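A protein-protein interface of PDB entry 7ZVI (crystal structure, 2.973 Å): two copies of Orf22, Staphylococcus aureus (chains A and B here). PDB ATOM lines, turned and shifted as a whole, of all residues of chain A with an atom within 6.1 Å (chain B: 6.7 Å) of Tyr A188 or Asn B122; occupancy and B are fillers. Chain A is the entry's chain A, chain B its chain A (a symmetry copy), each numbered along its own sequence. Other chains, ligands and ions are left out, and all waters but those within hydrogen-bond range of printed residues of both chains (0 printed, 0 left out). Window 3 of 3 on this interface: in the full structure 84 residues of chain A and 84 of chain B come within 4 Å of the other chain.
The guanidinium group (NH2) of Arg A168 sits at hydrogen-bond distance from the backbone carbonyl oxygen (O) of Ile B129 (3.1 Å). The side-chain amide nitrogen (ND2) of Asn B122 lies close to the side-chain amino group (NZ) of Lys A185, at 3.2 Å. The side-chain amide nitrogen (NE2) of Gln B119 is in hydrogen-bond range of the side-chain sulfur (SD) of Met A187 (3.5 Å). The side-chain amide nitrogen (NE2) of Gln B119 sits at hydrogen-bond distance from the side-chain hydroxyl (OH) of Tyr A188 (3.4 Å). The side-chain amide oxygen (OD1) of Asn B132 sits at hydrogen-bond distance from the side-chain amide nitrogen (ND2) of Asn A191 (3.2 Å). SD of Met A187 lies close to O of Phe B226.
The guanidinium group (NH1) of Arg A168 lies within hydrogen-bond range of the backbone carbonyl oxygen (O) of Tyr A188, at 2.9 Å. The side-chain hydroxyl (OH) of Tyr A190 lies close to the guanidinium group (NH1) of Arg A168 (3.2 Å). The side-chain amide oxygen (OD1) of Asn A191 lies within hydrogen-bond range of the guanidinium group (NH1) of Arg A168, at 2.7 Å. ND2 of Asn B122 is in hydrogen-bond range of O of Lys B118, 3.1 Å away. OD1 of Asn B122 lies close to NZ of Lys B143 (3.2 Å). The backbone carbonyl oxygen (O) of Phe B223 sits at hydrogen-bond distance from the side-chain hydroxyl (OG1) of Thr B227.
CB of Phe A165 touches ND2 of Asn B132, at 3.7 Å. NH2 of Arg A168 touches OD1 of Asn B132, at 3.7 Å. Arg A168 touches Phe B223. NZ of Lys B118 touches CD of Lys A185, at 3.4 Å. Thr B141 touches Lys A185 (CB to CE, 3.9 Å). Met A187 touches Thr B227 (O to CG2, 3.4 Å). CZ of Tyr A188 touches ND2 of Asn B122 (3.5 Å). CE of Lys B143 touches OH of Tyr A189 (3.1 Å). CD1 of Phe B223 touches OH of Tyr A190, at 3.4 Å. Tyr A190 touches Phe B226.
Tyr A188 touches three residues of chain B. Printed residues of chain B within 4 Å of Asn A191: Asn B132 (3.2 Å). Asn B122 touches just these residues of chain A: Lys A185 and Tyr A188. Ser B123 touches none of the printed residues of chain A. Of the printed residues of chain A, Asn B132 touches Phe A165 (3.7 Å), Arg A168 (3.7 Å) and Asn A191 (3.2 Å). The nearest residue of chain B that does not touch Tyr A188 is Ile B129 (4.05 Å).
Printed residues of chain B that touch a printed residue of chain A: Lys B118, Gln B119, Asn B122, Ile B129, Asn B132, Thr B141, Lys B143, Phe B223, Phe B226 and Thr B227. Of the 9 printed residues of chain A, 8 touch a printed residue of chain B. Printed residues of chain A that touch a printed residue of chain B: Phe A165, Arg A168, Lys A185, Met A187, Tyr A188, Tyr A189, Tyr A190 and Asn A191. Hydrophobic or aromatic side chains of chain A within 4 Å of the printed part of chain B: Phe A165, Met A187, Tyr A188, Tyr A189 and Tyr A190. Among the printed residues, 17 pairs touch across the chains. Among the printed residues, no Asp or Glu carboxylate lies within 4 Å of a Lys or Arg side-chain nitrogen of the other chain.
No position is printed for both chains. Of the 17 pairs that touch across the chains among the printed residues, none has its exchanged pair printed and touching as well.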
ATOM      1  N   PHE A 165      -7.167 -10.897  24.801  1.00  0.00           N
ATOM      2  CA  PHE A 165      -7.676  -9.824  23.907  1.00  0.00           C
ATOM      3  C   PHE A 165      -7.684  -8.487  24.650  1.00  0.00           C
ATOM      4  O   PHE A 165      -7.459  -8.457  25.877  1.00  0.00           O
ATOM      5  CB  PHE A 165      -9.103 -10.118  23.432  1.00  0.00           C
ATOM      6  CG  PHE A 165      -9.289 -11.433  22.721  1.00  0.00           C
ATOM      7  CD1 PHE A 165      -8.910 -11.584  21.396  1.00  0.00           C
ATOM      8  CD2 PHE A 165      -9.855 -12.516  23.374  1.00  0.00           C
ATOM      9  CE1 PHE A 165      -9.083 -12.793  20.743  1.00  0.00           C
ATOM     10  CE2 PHE A 165     -10.028 -13.726  22.720  1.00  0.00           C
ATOM     11  CZ  PHE A 165      -9.641 -13.863  21.405  1.00  0.00           C
ATOM     12  N   ARG A 168     -12.313  -4.170  21.058  1.00  0.00           N
ATOM     13  CA  ARG A 168     -12.096  -4.098  19.589  1.00  0.00           C
ATOM     14  C   ARG A 168     -11.783  -2.651  19.183  1.00  0.00           C
ATOM     15  O   ARG A 168     -12.358  -2.179  18.182  1.00  0.00           O
ATOM     16  CB  ARG A 168     -13.288  -4.713  18.852  1.00  0.00           C
ATOM     17  CG  ARG A 168     -13.340  -6.228  18.976  1.00  0.00           C
ATOM     18  CD  ARG A 168     -14.250  -6.878  17.960  1.00  0.00           C
ATOM     19  NE  ARG A 168     -14.126  -8.329  18.009  1.00  0.00           N
ATOM     20  CZ  ARG A 168     -13.171  -9.044  17.421  1.00  0.00           C
ATOM     21  NH1 ARG A 168     -12.224  -8.452  16.711  1.00  0.00           N
ATOM     22  NH2 ARG A 168     -13.172 -10.361  17.541  1.00  0.00           N
ATOM     23  N   LYS A 185      -7.717 -16.060   9.161  1.00  0.00           N
ATOM     24  CA  LYS A 185      -8.631 -16.046  10.334  1.00  0.00           C
ATOM     25  C   LYS A 185      -8.111 -15.110  11.437  1.00  0.00           C
ATOM     26  O   LYS A 185      -8.591 -15.233  12.579  1.00  0.00           O
ATOM     27  CB  LYS A 185      -8.802 -17.469  10.873  1.00  0.00           C
ATOM     28  CG  LYS A 185      -9.977 -18.245  10.295  1.00  0.00           C
ATOM     29  CD  LYS A 185     -10.521 -19.321  11.220  1.00  0.00           C
ATOM     30  CE  LYS A 185     -10.896 -18.828  12.605  1.00  0.00           C
ATOM     31  NZ  LYS A 185     -11.531 -17.488  12.591  1.00  0.00           N
ATOM     32  N   ASP A 186      -7.175 -14.212  11.115  1.00  0.00           N
ATOM     33  CA  ASP A 186      -6.706 -13.127  12.021  1.00  0.00           C
ATOM     34  C   ASP A 186      -7.199 -11.790  11.452  1.00  0.00           C
ATOM     35  O   ASP A 186      -6.600 -10.745  11.763  1.00  0.00           O
ATOM     36  CB  ASP A 186      -5.194 -13.218  12.237  1.00  0.00           C
ATOM     37  CG  ASP A 186      -4.774 -14.450  13.027  1.00  0.00           C
ATOM     38  OD1 ASP A 186      -5.659 -15.262  13.369  1.00  0.00           O
ATOM     39  OD2 ASP A 186      -3.565 -14.589  13.293  1.00  0.00           O
ATOM     40  N   MET A 187      -8.249 -11.858  10.626  1.00  0.00           N
ATOM     41  CA  MET A 187      -9.206 -10.756  10.343  1.00  0.00           C
ATOM     42  C   MET A 187     -10.310 -10.765  11.412  1.00  0.00           C
ATOM     43  O   MET A 187     -11.139  -9.837  11.407  1.00  0.00           O
ATOM     44  CB  MET A 187      -9.830 -10.909   8.950  1.00  0.00           C
ATOM     45  CG  MET A 187     -10.649 -12.182   8.765  1.00  0.00           C
ATOM     46  SD  MET A 187     -10.627 -12.812   7.061  1.00  0.00           S
ATOM     47  CE  MET A 187      -8.905 -13.284   6.899  1.00  0.00           C
ATOM     48  N   TYR A 188     -10.322 -11.780  12.284  1.00  0.00           N
ATOM     49  CA  TYR A 188     -11.227 -11.901  13.459  1.00  0.00           C
ATOM     50  C   TYR A 188     -10.477 -11.533  14.746  1.00  0.00           C
ATOM     51  O   TYR A 188     -11.028 -10.771  15.564  1.00  0.00           O
ATOM     52  CB  TYR A 188     -11.787 -13.322  13.560  1.00  0.00           C
ATOM     53  CG  TYR A 188     -12.717 -13.709  12.438  1.00  0.00           C
ATOM     54  CD1 TYR A 188     -12.235 -14.290  11.276  1.00  0.00           C
ATOM     55  CD2 TYR A 188     -14.081 -13.488  12.535  1.00  0.00           C
ATOM     56  CE1 TYR A 188     -13.086 -14.641  10.240  1.00  0.00           C
ATOM     57  CE2 TYR A 188     -14.945 -13.834  11.510  1.00  0.00           C
ATOM     58  CZ  TYR A 188     -14.446 -14.409  10.356  1.00  0.00           C
ATOM     59  OH  TYR A 188     -15.295 -14.750   9.342  1.00  0.00           O
ATOM     60  N   TYR A 189      -9.264 -12.068  14.920  1.00  0.00           N
ATOM     61  CA  TYR A 189      -8.457 -11.980  16.165  1.00  0.00           C
ATOM     62  C   TYR A 189      -7.237 -11.079  15.937  1.00  0.00           C
ATOM     63  O   TYR A 189      -6.087 -11.562  15.996  1.00  0.00           O
ATOM     64  CB  TYR A 189      -8.071 -13.387  16.624  1.00  0.00           C
ATOM     65  CG  TYR A 189      -9.177 -14.400  16.499  1.00  0.00           C
ATOM     66  CD1 TYR A 189     -10.386 -14.224  17.153  1.00  0.00           C
ATOM     67  CD2 TYR A 189      -9.017 -15.537  15.726  1.00  0.00           C
ATOM     68  CE1 TYR A 189     -11.408 -15.154  17.043  1.00  0.00           C
ATOM     69  CE2 TYR A 189     -10.027 -16.478  15.607  1.00  0.00           C
ATOM     70  CZ  TYR A 189     -11.227 -16.284  16.267  1.00  0.00           C
ATOM     71  OH  TYR A 189     -12.218 -17.212  16.146  1.00  0.00           O
ATOM     72  N   TYR A 190      -7.501  -9.792  15.694  1.00  0.00           N
ATOM     73  CA  TYR A 190      -6.502  -8.690  15.635  1.00  0.00           C
ATOM     74  C   TYR A 190      -6.409  -8.027  17.017  1.00  0.00           C
ATOM     75  O   TYR A 190      -5.596  -7.099  17.181  1.00  0.00           O
ATOM     76  CB  TYR A 190      -6.874  -7.679  14.547  1.00  0.00           C
ATOM     77  CG  TYR A 190      -8.297  -7.185  14.606  1.00  0.00           C
ATOM     78  CD1 TYR A 190      -8.652  -6.129  15.428  1.00  0.00           C
ATOM     79  CD2 TYR A 190      -9.296  -7.781  13.852  1.00  0.00           C
ATOM     80  CE1 TYR A 190      -9.959  -5.675  15.497  1.00  0.00           C
ATOM     81  CE2 TYR A 190     -10.609  -7.342  13.912  1.00  0.00           C
ATOM     82  CZ  TYR A 190     -10.942  -6.281  14.735  1.00  0.00           C
ATOM     83  OH  TYR A 190     -12.228  -5.830  14.809  1.00  0.00           O
ATOM     84  N   ASN A 191      -7.209  -8.508  17.978  1.00  0.00           N
ATOM     85  CA  ASN A 191      -7.320  -7.956  19.356  1.00  0.00           C
ATOM     86  C   ASN A 191      -6.313  -8.650  20.272  1.00  0.00           C
ATOM     87  O   ASN A 191      -6.163  -8.192  21.419  1.00  0.00           O
ATOM     88  CB  ASN A 191      -8.715  -8.133  19.965  1.00  0.00           C
ATOM     89  CG  ASN A 191      -9.778  -8.520  18.959  1.00  0.00           C
ATOM     90  OD1 ASN A 191      -9.862  -7.938  17.881  1.00  0.00           O
ATOM     91  ND2 ASN A 191     -10.587  -9.512  19.299  1.00  0.00           N
ATOM     92  N   ILE B 115     -11.472 -22.445   4.376  1.00  0.00           N
ATOM     93  CA  ILE B 115     -11.588 -21.038   4.868  1.00  0.00           C
ATOM     94  C   ILE B 115     -13.066 -20.638   4.865  1.00  0.00           C
ATOM     95  O   ILE B 115     -13.541 -20.145   5.901  1.00  0.00           O
ATOM     96  CB  ILE B 115     -10.739 -20.067   4.019  1.00  0.00           C
ATOM     97  CG1 ILE B 115      -9.241 -20.228   4.288  1.00  0.00           C
ATOM     98  CG2 ILE B 115     -11.190 -18.626   4.223  1.00  0.00           C
ATOM     99  CD1 ILE B 115      -8.795 -19.742   5.650  1.00  0.00           C
ATOM    100  N   LYS B 117     -15.887 -22.411   4.836  1.00  0.00           N
ATOM    101  CA  LYS B 117     -16.628 -23.188   5.869  1.00  0.00           C
ATOM    102  C   LYS B 117     -16.412 -22.526   7.234  1.00  0.00           C
ATOM    103  O   LYS B 117     -17.414 -22.212   7.901  1.00  0.00           O
ATOM    104  CB  LYS B 117     -16.172 -24.650   5.899  1.00  0.00           C
ATOM    105  CG  LYS B 117     -16.494 -25.462   4.650  1.00  0.00           C
ATOM    106  CD  LYS B 117     -17.925 -25.953   4.586  1.00  0.00           C
ATOM    107  CE  LYS B 117     -18.387 -26.258   3.176  1.00  0.00           C
ATOM    108  NZ  LYS B 117     -17.449 -27.159   2.462  1.00  0.00           N
ATOM    109  N   LYS B 118     -15.147 -22.308   7.610  1.00  0.00           N
ATOM    110  CA  LYS B 118     -14.741 -21.689   8.902  1.00  0.00           C
ATOM    111  C   LYS B 118     -15.449 -20.338   9.074  1.00  0.00           C
ATOM    112  O   LYS B 118     -16.031 -20.118  10.155  1.00  0.00           O
ATOM    113  CB  LYS B 118     -13.217 -21.528   8.972  1.00  0.00           C
ATOM    114  CG  LYS B 118     -12.432 -22.779   9.355  1.00  0.00           C
ATOM    115  CD  LYS B 118     -12.911 -23.476  10.619  1.00  0.00           C
ATOM    116  CE  LYS B 118     -13.041 -22.566  11.825  1.00  0.00           C
ATOM    117  NZ  LYS B 118     -11.719 -22.228  12.400  1.00  0.00           N
ATOM    118  N   GLN B 119     -15.409 -19.480   8.049  1.00  0.00           N
ATOM    119  CA  GLN B 119     -15.972 -18.100   8.079  1.00  0.00           C
ATOM    120  C   GLN B 119     -17.499 -18.154   8.190  1.00  0.00           C
ATOM    121  O   GLN B 119     -18.064 -17.299   8.899  1.00  0.00           O
ATOM    122  CB  GLN B 119     -15.559 -17.313   6.836  1.00  0.00           C
ATOM    123  CG  GLN B 119     -14.113 -16.845   6.872  1.00  0.00           C
ATOM    124  CD  GLN B 119     -13.860 -15.744   5.873  1.00  0.00           C
ATOM    125  OE1 GLN B 119     -13.863 -15.968   4.665  1.00  0.00           O
ATOM    126  NE2 GLN B 119     -13.640 -14.538   6.376  1.00  0.00           N
ATOM    127  N   ASN B 120     -18.134 -19.106   7.500  1.00  0.00           N
ATOM    128  CA  ASN B 120     -19.593 -19.380   7.602  1.00  0.00           C
ATOM    129  C   ASN B 120     -19.930 -19.733   9.056  1.00  0.00           C
ATOM    130  O   ASN B 120     -20.914 -19.178   9.582  1.00  0.00           O
ATOM    131  CB  ASN B 120     -20.033 -20.489   6.640  1.00  0.00           C
ATOM    132  CG  ASN B 120     -21.531 -20.706   6.619  1.00  0.00           C
ATOM    133  OD1 ASN B 120     -22.303 -19.814   6.969  1.00  0.00           O
ATOM    134  ND2 ASN B 120     -21.956 -21.889   6.203  1.00  0.00           N
ATOM    135  N   GLU B 121     -19.130 -20.608   9.679  1.00  0.00           N
ATOM    136  CA  GLU B 121     -19.339 -21.105  11.068  1.00  0.00           C
ATOM    137  C   GLU B 121     -19.096 -19.970  12.072  1.00  0.00           C
ATOM    138  O   GLU B 121     -19.784 -19.958  13.111  1.00  0.00           O
ATOM    139  CB  GLU B 121     -18.430 -22.301  11.366  1.00  0.00           C
ATOM    140  CG  GLU B 121     -18.702 -23.523  10.500  1.00  0.00           C
ATOM    141  CD  GLU B 121     -20.150 -23.981  10.423  1.00  0.00           C
ATOM    142  OE1 GLU B 121     -20.875 -23.847  11.432  1.00  0.00           O
ATOM    143  OE2 GLU B 121     -20.552 -24.474   9.348  1.00  0.00           O
ATOM    144  N   ASN B 122     -18.155 -19.066  11.778  1.00  0.00           N
ATOM    145  CA  ASN B 122     -17.872 -17.853  12.594  1.00  0.00           C
ATOM    146  C   ASN B 122     -19.068 -16.901  12.522  1.00  0.00           C
ATOM    147  O   ASN B 122     -19.519 -16.441  13.588  1.00  0.00           O
ATOM    148  CB  ASN B 122     -16.618 -17.110  12.131  1.00  0.00           C
ATOM    149  CG  ASN B 122     -15.357 -17.925  12.302  1.00  0.00           C
ATOM    150  OD1 ASN B 122     -15.221 -18.672  13.266  1.00  0.00           O
ATOM    151  ND2 ASN B 122     -14.436 -17.800  11.362  1.00  0.00           N
ATOM    152  N   SER B 123     -19.546 -16.624  11.305  1.00  0.00           N
ATOM    153  CA  SER B 123     -20.678 -15.706  11.008  1.00  0.00           C
ATOM    154  C   SER B 123     -21.867 -16.022  11.926  1.00  0.00           C
ATOM    155  O   SER B 123     -22.519 -15.068  12.386  1.00  0.00           O
ATOM    156  CB  SER B 123     -21.073 -15.781   9.554  1.00  0.00           C
ATOM    157  OG  SER B 123     -21.785 -14.616   9.164  1.00  0.00           O
ATOM    158  N   LYS B 124     -22.122 -17.312  12.182  1.00  0.00           N
ATOM    159  CA  LYS B 124     -23.227 -17.814  13.047  1.00  0.00           C
ATOM    160  C   LYS B 124     -23.057 -17.293  14.480  1.00  0.00           C
ATOM    161  O   LYS B 124     -24.086 -17.023  15.130  1.00  0.00           O
ATOM    162  CB  LYS B 124     -23.261 -19.345  13.054  1.00  0.00           C
ATOM    163  CG  LYS B 124     -23.619 -19.997  11.725  1.00  0.00           C
ATOM    164  CD  LYS B 124     -23.393 -21.496  11.711  1.00  0.00           C
ATOM    165  CE  LYS B 124     -23.588 -22.121  10.345  1.00  0.00           C
ATOM    166  NZ  LYS B 124     -25.017 -22.141   9.946  1.00  0.00           N
ATOM    167  N   ILE B 125     -21.810 -17.167  14.949  1.00  0.00           N
ATOM    168  CA  ILE B 125     -21.460 -16.752  16.342  1.00  0.00           C
ATOM    169  C   ILE B 125     -20.704 -15.416  16.309  1.00  0.00           C
ATOM    170  O   ILE B 125     -19.901 -15.171  17.234  1.00  0.00           O
ATOM    171  CB  ILE B 125     -20.652 -17.861  17.046  1.00  0.00           C
ATOM    172  CG1 ILE B 125     -19.358 -18.199  16.298  1.00  0.00           C
ATOM    173  CG2 ILE B 125     -21.521 -19.091  17.256  1.00  0.00           C
ATOM    174  CD1 ILE B 125     -18.345 -18.959  17.125  1.00  0.00           C
ATOM    175  N   GLU B 126     -20.966 -14.581  15.298  1.00  0.00           N
ATOM    176  CA  GLU B 126     -20.342 -13.239  15.130  1.00  0.00           C
ATOM    177  C   GLU B 126     -20.518 -12.443  16.429  1.00  0.00           C
ATOM    178  O   GLU B 126     -19.566 -11.744  16.826  1.00  0.00           O
ATOM    179  CB  GLU B 126     -20.962 -12.505  13.940  1.00  0.00           C
ATOM    180  CG  GLU B 126     -20.139 -11.325  13.460  1.00  0.00           C
ATOM    181  CD  GLU B 126     -20.739 -10.576  12.283  1.00  0.00           C
ATOM    182  OE1 GLU B 126     -21.010 -11.223  11.248  1.00  0.00           O
ATOM    183  OE2 GLU B 126     -20.938  -9.351  12.401  1.00  0.00           O
ATOM    184  N   SER B 127     -21.694 -12.562  17.055  1.00  0.00           N
ATOM    185  CA  SER B 127     -22.041 -11.981  18.380  1.00  0.00           C
ATOM    186  C   SER B 127     -20.910 -12.239  19.383  1.00  0.00           C
ATOM    187  O   SER B 127     -20.277 -11.260  19.825  1.00  0.00           O
ATOM    188  CB  SER B 127     -23.363 -12.531  18.876  1.00  0.00           C
ATOM    189  OG  SER B 127     -23.485 -12.407  20.286  1.00  0.00           O
ATOM    190  N   ILE B 129     -17.954 -13.879  19.085  1.00  0.00           N
ATOM    191  CA  ILE B 129     -16.609 -13.548  18.525  1.00  0.00           C
ATOM    192  C   ILE B 129     -16.354 -12.059  18.761  1.00  0.00           C
ATOM    193  O   ILE B 129     -15.297 -11.733  19.337  1.00  0.00           O
ATOM    194  CB  ILE B 129     -16.488 -13.931  17.035  1.00  0.00           C
ATOM    195  CG1 ILE B 129     -16.303 -15.441  16.864  1.00  0.00           C
ATOM    196  CG2 ILE B 129     -15.367 -13.152  16.360  1.00  0.00           C
ATOM    197  CD1 ILE B 129     -16.368 -15.917  15.430  1.00  0.00           C
ATOM    198  N   ASN B 132     -15.979 -10.826  22.307  1.00  0.00           N
ATOM    199  CA  ASN B 132     -14.776 -11.499  22.868  1.00  0.00           C
ATOM    200  C   ASN B 132     -15.194 -12.569  23.888  1.00  0.00           C
ATOM    201  O   ASN B 132     -14.345 -12.939  24.732  1.00  0.00           O
ATOM    202  CB  ASN B 132     -13.785 -10.491  23.463  1.00  0.00           C
ATOM    203  CG  ASN B 132     -13.102  -9.634  22.417  1.00  0.00           C
ATOM    204  OD1 ASN B 132     -13.143  -9.936  21.226  1.00  0.00           O
ATOM    205  ND2 ASN B 132     -12.461  -8.563  22.854  1.00  0.00           N
ATOM    206  N   THR B 141      -6.041 -20.949  15.848  1.00  0.00           N
ATOM    207  CA  THR B 141      -7.346 -20.309  15.526  1.00  0.00           C
ATOM    208  C   THR B 141      -8.475 -21.152  16.140  1.00  0.00           C
ATOM    209  O   THR B 141      -9.649 -20.759  15.987  1.00  0.00           O
ATOM    210  CB  THR B 141      -7.543 -20.140  14.013  1.00  0.00           C
ATOM    211  OG1 THR B 141      -7.957 -21.390  13.459  1.00  0.00           O
ATOM    212  CG2 THR B 141      -6.305 -19.654  13.291  1.00  0.00           C
ATOM    213  N   LYS B 143     -10.962 -22.352  18.812  1.00  0.00           N
ATOM    214  CA  LYS B 143     -11.696 -21.512  19.796  1.00  0.00           C
ATOM    215  C   LYS B 143     -12.892 -22.286  20.347  1.00  0.00           C
ATOM    216  O   LYS B 143     -13.369 -23.218  19.669  1.00  0.00           O
ATOM    217  CB  LYS B 143     -12.214 -20.228  19.141  1.00  0.00           C
ATOM    218  CG  LYS B 143     -12.829 -20.420  17.761  1.00  0.00           C
ATOM    219  CD  LYS B 143     -13.985 -19.498  17.461  1.00  0.00           C
ATOM    220  CE  LYS B 143     -14.348 -19.480  15.992  1.00  0.00           C
ATOM    221  NZ  LYS B 143     -14.512 -20.846  15.442  1.00  0.00           N
ATOM    222  N   PHE B 223     -14.702  -4.121  12.049  1.00  0.00           N
ATOM    223  CA  PHE B 223     -14.832  -5.591  12.216  1.00  0.00           C
ATOM    224  C   PHE B 223     -15.674  -6.167  11.071  1.00  0.00           C
ATOM    225  O   PHE B 223     -15.231  -7.146  10.446  1.00  0.00           O
ATOM    226  CB  PHE B 223     -15.440  -5.909  13.585  1.00  0.00           C
ATOM    227  CG  PHE B 223     -15.685  -7.372  13.850  1.00  0.00           C
ATOM    228  CD1 PHE B 223     -14.672  -8.191  14.324  1.00  0.00           C
ATOM    229  CD2 PHE B 223     -16.935  -7.929  13.632  1.00  0.00           C
ATOM    230  CE1 PHE B 223     -14.902  -9.536  14.567  1.00  0.00           C
ATOM    231  CE2 PHE B 223     -17.163  -9.273  13.878  1.00  0.00           C
ATOM    232  CZ  PHE B 223     -16.149 -10.074  14.346  1.00  0.00           C
ATOM    233  N   PHE B 226     -13.940  -6.350   7.759  1.00  0.00           N
ATOM    234  CA  PHE B 226     -12.747  -7.234   7.873  1.00  0.00           C
ATOM    235  C   PHE B 226     -13.169  -8.700   7.710  1.00  0.00           C
ATOM    236  O   PHE B 226     -12.407  -9.481   7.106  1.00  0.00           O
ATOM    237  CB  PHE B 226     -12.033  -7.037   9.215  1.00  0.00           C
ATOM    238  CG  PHE B 226     -10.525  -6.997   9.155  1.00  0.00           C
ATOM    239  CD1 PHE B 226      -9.822  -7.528   8.083  1.00  0.00           C
ATOM    240  CD2 PHE B 226      -9.803  -6.437  10.198  1.00  0.00           C
ATOM    241  CE1 PHE B 226      -8.436  -7.485   8.051  1.00  0.00           C
ATOM    242  CE2 PHE B 226      -8.416  -6.399  10.166  1.00  0.00           C
ATOM    243  CZ  PHE B 226      -7.736  -6.923   9.092  1.00  0.00           C
ATOM    244  N   THR B 227     -14.345  -9.054   8.240  1.00  0.00           N
ATOM    245  CA  THR B 227     -14.913 -10.429   8.247  1.00  0.00           C
ATOM    246  C   THR B 227     -16.039 -10.514   7.209  1.00  0.00           C
ATOM    247  O   THR B 227     -17.150 -10.046   7.515  1.00  0.00           O
ATOM    248  CB  THR B 227     -15.401 -10.810   9.652  1.00  0.00           C
ATOM    249  OG1 THR B 227     -16.527 -10.003  10.006  1.00  0.00           O
ATOM    250  CG2 THR B 227     -14.333 -10.647  10.711  1.00  0.00           C
ATOM    251  N   ASN B 228     -15.755 -11.081   6.031  1.00  0.00           N
ATOM    252  CA  ASN B 228     -16.740 -11.280   4.930  1.00  0.00           C
ATOM    253  C   ASN B 228     -16.058 -11.966   3.738  1.00  0.00           C
ATOM    254  O   ASN B 228     -14.851 -12.268   3.838  1.00  0.00           O
ATOM    255  CB  ASN B 228     -17.399  -9.960   4.508  1.00  0.00           C
ATOM    256  CG  ASN B 228     -16.404  -8.895   4.100  1.00  0.00           C
ATOM    257  OD1 ASN B 228     -15.200  -9.142   4.046  1.00  0.00           O
ATOM    258  ND2 ASN B 228     -16.898  -7.703   3.809  1.00  0.00           N
